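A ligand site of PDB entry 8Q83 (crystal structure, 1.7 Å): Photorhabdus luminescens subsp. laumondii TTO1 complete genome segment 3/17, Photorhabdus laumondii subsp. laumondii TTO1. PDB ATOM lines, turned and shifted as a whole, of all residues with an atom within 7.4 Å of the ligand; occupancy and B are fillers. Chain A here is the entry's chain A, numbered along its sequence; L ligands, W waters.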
ATOM      1  N   ASN A 135      -0.154 -10.995   4.025  1.00  0.00           N
ATOM      2  CA  ASN A 135      -1.300 -11.718   4.639  1.00  0.00           C
ATOM      3  C   ASN A 135      -1.835 -12.756   3.640  1.00  0.00           C
ATOM      4  O   ASN A 135      -1.502 -12.701   2.436  1.00  0.00           O
ATOM      5  CB  ASN A 135      -2.412 -10.759   5.050  1.00  0.00           C
ATOM      6  CG  ASN A 135      -2.141 -10.064   6.368  1.00  0.00           C
ATOM      7  OD1 ASN A 135      -2.360 -10.622   7.438  1.00  0.00           O
ATOM      8  ND2 ASN A 135      -1.687  -8.818   6.293  1.00  0.00           N
ATOM      9  N   ASP A 137      -4.549 -12.838   2.380  1.00  0.00           N
ATOM     10  CA  ASP A 137      -5.421 -12.099   1.417  1.00  0.00           C
ATOM     11  C   ASP A 137      -4.580 -11.212   0.463  1.00  0.00           C
ATOM     12  O   ASP A 137      -5.202 -10.372  -0.242  1.00  0.00           O
ATOM     13  CB  ASP A 137      -6.472 -11.290   2.175  1.00  0.00           C
ATOM     14  CG  ASP A 137      -5.922 -10.163   3.040  1.00  0.00           C
ATOM     15  OD1 ASP A 137      -4.692  -9.983   3.079  1.00  0.00           O
ATOM     16  OD2 ASP A 137      -6.740  -9.462   3.677  1.00  0.00           O
ATOM     17  N   ARG A 139      -2.461  -8.762   1.146  1.00  0.00           N
ATOM     18  CA  ARG A 139      -2.129  -7.408   1.672  1.00  0.00           C
ATOM     19  C   ARG A 139      -0.801  -7.471   2.421  1.00  0.00           C
ATOM     20  O   ARG A 139      -0.696  -8.272   3.364  1.00  0.00           O
ATOM     21  CB  ARG A 139      -3.228  -6.885   2.606  1.00  0.00           C
ATOM     22  CG  ARG A 139      -4.473  -6.343   1.908  1.00  0.00           C
ATOM     23  CD  ARG A 139      -5.592  -5.952   2.863  1.00  0.00           C
ATOM     24  NE  ARG A 139      -5.735  -6.935   3.919  1.00  0.00           N
ATOM     25  CZ  ARG A 139      -5.203  -6.817   5.140  1.00  0.00           C
ATOM     26  NH1 ARG A 139      -4.550  -5.713   5.498  1.00  0.00           N
ATOM     27  NH2 ARG A 139      -5.348  -7.790   6.018  1.00  0.00           N
ATOM     28  N   LEU A 140       0.189  -6.686   2.006  1.00  0.00           N
ATOM     29  CA  LEU A 140       1.431  -6.465   2.788  1.00  0.00           C
ATOM     30  C   LEU A 140       1.096  -5.812   4.133  1.00  0.00           C
ATOM     31  O   LEU A 140       0.116  -5.028   4.238  1.00  0.00           O
ATOM     32  CB  LEU A 140       2.403  -5.592   1.987  1.00  0.00           C
ATOM     33  CG  LEU A 140       2.850  -6.163   0.645  1.00  0.00           C
ATOM     34  CD1 LEU A 140       4.031  -5.369   0.120  1.00  0.00           C
ATOM     35  CD2 LEU A 140       3.188  -7.638   0.750  1.00  0.00           C
ATOM     36  N   GLU A 141       1.921  -6.113   5.119  1.00  0.00           N
ATOM     37  CA  GLU A 141       1.780  -5.600   6.492  1.00  0.00           C
ATOM     38  C   GLU A 141       3.199  -5.405   7.016  1.00  0.00           C
ATOM     39  O   GLU A 141       4.028  -6.337   6.881  1.00  0.00           O
ATOM     40  CB  GLU A 141       0.931  -6.534   7.347  1.00  0.00           C
ATOM     41  CG  GLU A 141       0.500  -5.940   8.668  1.00  0.00           C
ATOM     42  CD  GLU A 141      -0.691  -6.594   9.345  1.00  0.00           C
ATOM     43  OE1 GLU A 141      -1.521  -7.181   8.637  1.00  0.00           O
ATOM     44  OE2 GLU A 141      -0.787  -6.510  10.586  1.00  0.00           O
ATOM     45  N   PHE A 143       5.816  -4.018  10.177  1.00  0.00           N
ATOM     46  CA  PHE A 143       5.984  -4.014  11.647  1.00  0.00           C
ATOM     47  C   PHE A 143       7.282  -3.268  11.952  1.00  0.00           C
ATOM     48  O   PHE A 143       8.286  -3.479  11.263  1.00  0.00           O
ATOM     49  CB  PHE A 143       6.005  -5.451  12.171  1.00  0.00           C
ATOM     50  CG  PHE A 143       4.761  -6.241  11.857  1.00  0.00           C
ATOM     51  CD1 PHE A 143       4.662  -6.965  10.677  1.00  0.00           C
ATOM     52  CD2 PHE A 143       3.698  -6.241  12.731  1.00  0.00           C
ATOM     53  CE1 PHE A 143       3.501  -7.666  10.380  1.00  0.00           C
ATOM     54  CE2 PHE A 143       2.537  -6.942  12.434  1.00  0.00           C
ATOM     55  CZ  PHE A 143       2.443  -7.664  11.271  1.00  0.00           C
ATOM     56  N   HIS A 153       2.249  -1.451  13.759  1.00  0.00           N
ATOM     57  CA  HIS A 153       2.051  -2.063  12.425  1.00  0.00           C
ATOM     58  C   HIS A 153       1.117  -1.199  11.587  1.00  0.00           C
ATOM     59  O   HIS A 153       0.466  -0.286  12.142  1.00  0.00           O
ATOM     60  CB  HIS A 153       1.607  -3.524  12.556  1.00  0.00           C
ATOM     61  CG  HIS A 153       0.260  -3.755  13.154  1.00  0.00           C
ATOM     62  ND1 HIS A 153      -0.551  -4.774  12.693  1.00  0.00           N
ATOM     63  CD2 HIS A 153      -0.403  -3.164  14.178  1.00  0.00           C
ATOM     64  CE1 HIS A 153      -1.661  -4.801  13.403  1.00  0.00           C
ATOM     65  NE2 HIS A 153      -1.601  -3.813  14.315  1.00  0.00           N
ATOM     66  N   ILE A 154       1.134  -1.482  10.285  1.00  0.00           N
ATOM     67  CA  ILE A 154       0.450  -0.715   9.202  1.00  0.00           C
ATOM     68  C   ILE A 154       0.252  -1.704   8.057  1.00  0.00           C
ATOM     69  O   ILE A 154       1.020  -2.657   7.997  1.00  0.00           O
ATOM     70  CB  ILE A 154       1.295   0.511   8.806  1.00  0.00           C
ATOM     71  CG1 ILE A 154       0.496   1.502   7.951  1.00  0.00           C
ATOM     72  CG2 ILE A 154       2.595   0.075   8.135  1.00  0.00           C
ATOM     73  CD1 ILE A 154       1.275   2.716   7.491  1.00  0.00           C
ATOM     74  N   TRP A 155      -0.773  -1.532   7.222  1.00  0.00           N
ATOM     75  CA  TRP A 155      -1.062  -2.507   6.131  1.00  0.00           C
ATOM     76  C   TRP A 155      -1.659  -1.799   4.911  1.00  0.00           C
ATOM     77  O   TRP A 155      -2.335  -0.762   5.077  1.00  0.00           O
ATOM     78  CB  TRP A 155      -2.002  -3.619   6.615  1.00  0.00           C
ATOM     79  CG  TRP A 155      -3.210  -3.089   7.336  1.00  0.00           C
ATOM     80  CD1 TRP A 155      -4.405  -2.750   6.778  1.00  0.00           C
ATOM     81  CD2 TRP A 155      -3.310  -2.792   8.739  1.00  0.00           C
ATOM     82  NE1 TRP A 155      -5.261  -2.285   7.744  1.00  0.00           N
ATOM     83  CE2 TRP A 155      -4.620  -2.313   8.950  1.00  0.00           C
ATOM     84  CE3 TRP A 155      -2.460  -2.914   9.840  1.00  0.00           C
ATOM     85  CZ2 TRP A 155      -5.085  -1.929  10.212  1.00  0.00           C
ATOM     86  CZ3 TRP A 155      -2.912  -2.535  11.087  1.00  0.00           C
ATOM     87  CH2 TRP A 155      -4.208  -2.056  11.270  1.00  0.00           C
ATOM     88  N   GLN A 156      -1.351  -2.336   3.737  1.00  0.00           N
ATOM     89  CA  GLN A 156      -2.150  -2.158   2.503  1.00  0.00           C
ATOM     90  C   GLN A 156      -3.619  -2.397   2.882  1.00  0.00           C
ATOM     91  O   GLN A 156      -3.914  -3.423   3.545  1.00  0.00           O
ATOM     92  CB  GLN A 156      -1.745  -3.134   1.402  1.00  0.00           C
ATOM     93  CG  GLN A 156      -0.372  -2.826   0.803  1.00  0.00           C
ATOM     94  CD  GLN A 156       0.113  -3.819  -0.227  1.00  0.00           C
ATOM     95  OE1 GLN A 156      -0.361  -4.953  -0.334  1.00  0.00           O
ATOM     96  NE2 GLN A 156       1.093  -3.384  -1.002  1.00  0.00           N
ATOM     97  N   THR A 157      -4.497  -1.477   2.474  1.00  0.00           N
ATOM     98  CA  THR A 157      -5.968  -1.583   2.680  1.00  0.00           C
ATOM     99  C   THR A 157      -6.595  -2.524   1.644  1.00  0.00           C
ATOM    100  O   THR A 157      -7.724  -3.011   1.911  1.00  0.00           O
ATOM    101  CB  THR A 157      -6.622  -0.197   2.643  1.00  0.00           C
ATOM    102  OG1 THR A 157      -6.226   0.437   1.432  1.00  0.00           O
ATOM    103  CG2 THR A 157      -6.249   0.659   3.839  1.00  0.00           C
ATOM    104  N   SER A 165      -3.371   1.769   5.646  1.00  0.00           N
ATOM    105  CA  SER A 165      -3.923   2.146   6.970  1.00  0.00           C
ATOM    106  C   SER A 165      -3.046   3.251   7.581  1.00  0.00           C
ATOM    107  O   SER A 165      -1.923   3.499   7.044  1.00  0.00           O
ATOM    108  CB  SER A 165      -3.992   0.944   7.870  1.00  0.00           C
ATOM    109  OG  SER A 165      -2.687   0.636   8.391  1.00  0.00           O
ATOM    110  N   TYR A 168      -1.019   1.656  14.118  1.00  0.00           N
ATOM    111  CA  TYR A 168      -1.627   1.062  15.341  1.00  0.00           C
ATOM    112  C   TYR A 168      -0.505   0.444  16.172  1.00  0.00           C
ATOM    113  O   TYR A 168       0.473  -0.056  15.584  1.00  0.00           O
ATOM    114  CB  TYR A 168      -2.716   0.069  14.962  1.00  0.00           C
ATOM    115  CG  TYR A 168      -3.855   0.697  14.207  1.00  0.00           C
ATOM    116  CD1 TYR A 168      -4.952   1.230  14.860  1.00  0.00           C
ATOM    117  CD2 TYR A 168      -3.803   0.823  12.830  1.00  0.00           C
ATOM    118  CE1 TYR A 168      -5.980   1.849  14.161  1.00  0.00           C
ATOM    119  CE2 TYR A 168      -4.812   1.435  12.108  1.00  0.00           C
ATOM    120  CZ  TYR A 168      -5.902   1.951  12.785  1.00  0.00           C
ATOM    121  OH  TYR A 168      -6.894   2.561  12.065  1.00  0.00           O
ATOM    122  N   LEU A 170       0.472  -2.527  18.917  1.00  0.00           N
ATOM    123  CA  LEU A 170       0.127  -3.839  19.500  1.00  0.00           C
ATOM    124  C   LEU A 170       0.652  -3.910  20.942  1.00  0.00           C
ATOM    125  O   LEU A 170       0.521  -4.964  21.562  1.00  0.00           O
ATOM    126  CB  LEU A 170       0.693  -4.952  18.613  1.00  0.00           C
ATOM    127  CG  LEU A 170      -0.103  -5.156  17.317  1.00  0.00           C
ATOM    128  CD1 LEU A 170       0.710  -5.899  16.275  1.00  0.00           C
ATOM    129  CD2 LEU A 170      -1.413  -5.872  17.606  1.00  0.00           C
ATOM    130  N   LEU A 188      -0.475 -14.264  10.731  1.00  0.00           N
ATOM    131  CA  LEU A 188       0.837 -13.593  10.922  1.00  0.00           C
ATOM    132  C   LEU A 188       1.252 -13.757  12.380  1.00  0.00           C
ATOM    133  O   LEU A 188       0.369 -13.762  13.258  1.00  0.00           O
ATOM    134  CB  LEU A 188       0.773 -12.105  10.561  1.00  0.00           C
ATOM    135  CG  LEU A 188       0.449 -11.784   9.108  1.00  0.00           C
ATOM    136  CD1 LEU A 188       0.582 -10.285   8.840  1.00  0.00           C
ATOM    137  CD2 LEU A 188       1.318 -12.588   8.157  1.00  0.00           C
ATOM    138  N   GLN A 204      -1.954 -12.944  14.968  1.00  0.00           N
ATOM    139  CA  GLN A 204      -3.369 -12.742  14.586  1.00  0.00           C
ATOM    140  C   GLN A 204      -4.188 -13.877  15.204  1.00  0.00           C
ATOM    141  O   GLN A 204      -3.658 -15.003  15.276  1.00  0.00           O
ATOM    142  CB  GLN A 204      -3.501 -12.658  13.067  1.00  0.00           C
ATOM    143  CG  GLN A 204      -2.786 -11.459  12.451  1.00  0.00           C
ATOM    144  CD  GLN A 204      -2.831 -11.428  10.940  1.00  0.00           C
ATOM    145  OE1 GLN A 204      -2.797 -12.447  10.262  1.00  0.00           O
ATOM    146  NE2 GLN A 204      -2.842 -10.222  10.385  1.00  0.00           N
ATOM    147  N   ALA A 206      -6.990 -15.052  13.932  1.00  0.00           N
ATOM    148  CA  ALA A 206      -7.197 -15.806  12.685  1.00  0.00           C
ATOM    149  C   ALA A 206      -6.631 -14.984  11.534  1.00  0.00           C
ATOM    150  O   ALA A 206      -6.351 -13.799  11.719  1.00  0.00           O
ATOM    151  CB  ALA A 206      -8.672 -16.092  12.514  1.00  0.00           C
ATOM    152  N   PRO A 207      -6.449 -15.545  10.315  1.00  0.00           N
ATOM    153  CA  PRO A 207      -5.825 -14.779   9.242  1.00  0.00           C
ATOM    154  C   PRO A 207      -6.504 -13.410   9.070  1.00  0.00           C
ATOM    155  O   PRO A 207      -7.721 -13.357   8.856  1.00  0.00           O
ATOM    156  CB  PRO A 207      -5.986 -15.694   8.014  1.00  0.00           C
ATOM    157  CG  PRO A 207      -6.048 -17.088   8.602  1.00  0.00           C
ATOM    158  CD  PRO A 207      -6.750 -16.933   9.932  1.00  0.00           C
ATOM    159  N   HIS A 208      -5.700 -12.342   9.178  1.00  0.00           N
ATOM    160  CA  HIS A 208      -6.156 -10.937   9.021  1.00  0.00           C
ATOM    161  C   HIS A 208      -7.568 -10.762   9.621  1.00  0.00           C
ATOM    162  O   HIS A 208      -8.432 -10.144   8.979  1.00  0.00           O
ATOM    163  CB  HIS A 208      -6.075 -10.551   7.539  1.00  0.00           C
ATOM    164  CG  HIS A 208      -6.698 -11.569   6.635  1.00  0.00           C
ATOM    165  ND1 HIS A 208      -8.041 -11.538   6.309  1.00  0.00           N
ATOM    166  CD2 HIS A 208      -6.188 -12.657   6.027  1.00  0.00           C
ATOM    167  CE1 HIS A 208      -8.321 -12.566   5.546  1.00  0.00           C
ATOM    168  NE2 HIS A 208      -7.215 -13.266   5.349  1.00  0.00           N
ATOM    169  N   SER A 209      -7.785 -11.286  10.831  1.00  0.00           N
ATOM    170  CA  SER A 209      -9.113 -11.308  11.517  1.00  0.00           C
ATOM    171  C   SER A 209      -9.544  -9.886  11.909  1.00  0.00           C
ATOM    172  O   SER A 209     -10.768  -9.642  12.007  1.00  0.00           O
ATOM    173  CB  SER A 209      -9.067 -12.188  12.727  1.00  0.00           C
ATOM    174  OG  SER A 209      -8.125 -11.687  13.660  1.00  0.00           O
ATOM    175  N   GLY A 210      -8.559  -9.008  12.155  1.00  0.00           N
ATOM    176  CA  GLY A 210      -8.754  -7.654  12.710  1.00  0.00           C
ATOM    177  C   GLY A 210      -8.397  -7.620  14.182  1.00  0.00           C
ATOM    178  O   GLY A 210      -8.499  -6.526  14.795  1.00  0.00           O
ATOM    179  N   TYR A 211      -7.948  -8.759  14.736  1.00  0.00           N
ATOM    180  CA  TYR A 211      -7.615  -8.940  16.170  1.00  0.00           C
ATOM    181  C   TYR A 211      -6.297  -9.693  16.310  1.00  0.00           C
ATOM    182  O   TYR A 211      -6.005 -10.571  15.500  1.00  0.00           O
ATOM    183  CB  TYR A 211      -8.712  -9.735  16.885  1.00  0.00           C
ATOM    184  CG  TYR A 211     -10.065  -9.094  16.749  1.00  0.00           C
ATOM    185  CD1 TYR A 211     -10.423  -8.024  17.541  1.00  0.00           C
ATOM    186  CD2 TYR A 211     -10.960  -9.507  15.777  1.00  0.00           C
ATOM    187  CE1 TYR A 211     -11.657  -7.408  17.418  1.00  0.00           C
ATOM    188  CE2 TYR A 211     -12.199  -8.903  15.626  1.00  0.00           C
ATOM    189  CZ  TYR A 211     -12.543  -7.843  16.446  1.00  0.00           C
ATOM    190  OH  TYR A 211     -13.753  -7.222  16.327  1.00  0.00           O
ATOM    191  N   TRP A 212      -5.543  -9.358  17.360  1.00  0.00           N
ATOM    192  CA  TRP A 212      -4.293 -10.071  17.737  1.00  0.00           C
ATOM    193  C   TRP A 212      -4.469 -10.672  19.136  1.00  0.00           C
ATOM    194  O   TRP A 212      -5.435 -10.313  19.828  1.00  0.00           O
ATOM    195  CB  TRP A 212      -3.072  -9.149  17.635  1.00  0.00           C
ATOM    196  CG  TRP A 212      -2.723  -8.818  16.219  1.00  0.00           C
ATOM    197  CD1 TRP A 212      -3.477  -8.106  15.335  1.00  0.00           C
ATOM    198  CD2 TRP A 212      -1.545  -9.227  15.505  1.00  0.00           C
ATOM    199  NE1 TRP A 212      -2.850  -8.036  14.118  1.00  0.00           N
ATOM    200  CE2 TRP A 212      -1.658  -8.706  14.195  1.00  0.00           C
ATOM    201  CE3 TRP A 212      -0.406  -9.979  15.841  1.00  0.00           C
ATOM    202  CZ2 TRP A 212      -0.672  -8.909  13.236  1.00  0.00           C
ATOM    203  CZ3 TRP A 212       0.574 -10.180  14.889  1.00  0.00           C
ATOM    204  CH2 TRP A 212       0.442  -9.653  13.603  1.00  0.00           C
HETATM  205  C1  LIG L   1      -6.175  -6.701   9.293  1.00  0.00           C
HETATM  206  C2  LIG L   1      -4.933  -7.420   9.826  1.00  0.00           C
HETATM  207  C3  LIG L   1      -4.072  -6.495  10.688  1.00  0.00           C
HETATM  208  C4  LIG L   1      -4.936  -5.757  11.715  1.00  0.00           C
HETATM  209  C5  LIG L   1      -6.111  -5.074  11.036  1.00  0.00           C
HETATM  210  C6  LIG L   1      -7.025  -4.315  11.988  1.00  0.00           C
HETATM  211  O1  LIG L   1      -5.818  -5.728   8.311  1.00  0.00           O
HETATM  212  O2  LIG L   1      -4.203  -7.982   8.730  1.00  0.00           O
HETATM  213  O3  LIG L   1      -3.047  -7.255  11.332  1.00  0.00           O
HETATM  214  O4  LIG L   1      -5.423  -6.658  12.729  1.00  0.00           O
HETATM  215  O5  LIG L   1      -6.875  -6.057  10.337  1.00  0.00           O
HETATM  216  C7  LIG L   1      -6.972  -5.117   7.722  1.00  0.00           C
HETATM  217  O   HOH W   1      -5.836  -5.529  15.216  1.00  0.00           O
HETATM  218  O   HOH W   2      -9.705  -5.780  10.116  1.00  0.00           O
HETATM  219  O   HOH W   3      -5.601  -9.606  12.629  1.00  0.00           O
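OE2 of Glu 141 sits at hydrogen-bond distance from O3 of the ligand (2.5 Å). NE1 of Trp 212 lies within hydrogen-bond range of O3 of the ligand (2.9 Å). NH2 of Arg 139 is in hydrogen-bond range of O2 of the ligand. The side-chain amide nitrogen of Gln 204 lies within hydrogen-bond range of an oxygen (O2) of the ligand. O2 of the ligand sits at hydrogen-bond distance from OD1 of Asn 135, at 3.5 Å.
The side-chain carboxylate (OE2) of Glu 141 lies within hydrogen-bond range of a ring nitrogen (ND1) of His 153, 2.7 Å away. The backbone carbonyl oxygen (O) of Arg 139 sits at hydrogen-bond distance from the side-chain amide nitrogen (ND2) of Asn 135 (3.1 Å). The guanidinium group of Arg 139 is in hydrogen-bond range of the backbone carbonyl oxygen of Gln 156. The guanidinium group (NE) of Arg 139 lies within salt-bridge range of the side-chain carboxylate (OD2) of Asp 137, 2.7 Å away. N of His 208 lies within hydrogen-bond range of OE1 of Gln 204, at 3.1 Å. The side-chain amide nitrogen of Gln 204 sits at hydrogen-bond distance from the side-chain amide oxygen of Asn 135, 3.0 Å away. The backbone carbonyl oxygen (O) of Trp 155 is in hydrogen-bond range of the backbone NH (N) of Ser 165 (2.8 Å). The backbone NH (N) of His 153 sits at hydrogen-bond distance from the backbone carbonyl oxygen (O) of Tyr 168 (2.9 Å).
His 153 touches the ligand. Trp 155 touches the ligand. His 208 touches the ligand. Gly 210 touches the ligand (CA to O5, 3.4 Å). Tyr 211 touches the ligand. Hydrophobic or aromatic side chains that line the ligand: His 153, Trp 155, His 208 and Trp 212. The nearest printed residue that does not touch the ligand is Ser 209 (4.9 Å).
Water W1 bridges an oxygen (O4) of the ligand (2.8 Å) and the backbone carbonyl oxygen of Gly 210 (2.9 Å). Water W3 lies within hydrogen-bond range of an oxygen (O4) of the ligand (3.0 Å), the backbone NH of Gly 210 (3.1 Å), the backbone carbonyl oxygen of Tyr 211 (3.1 Å) and the backbone NH of Ser 209 (3.3 Å).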
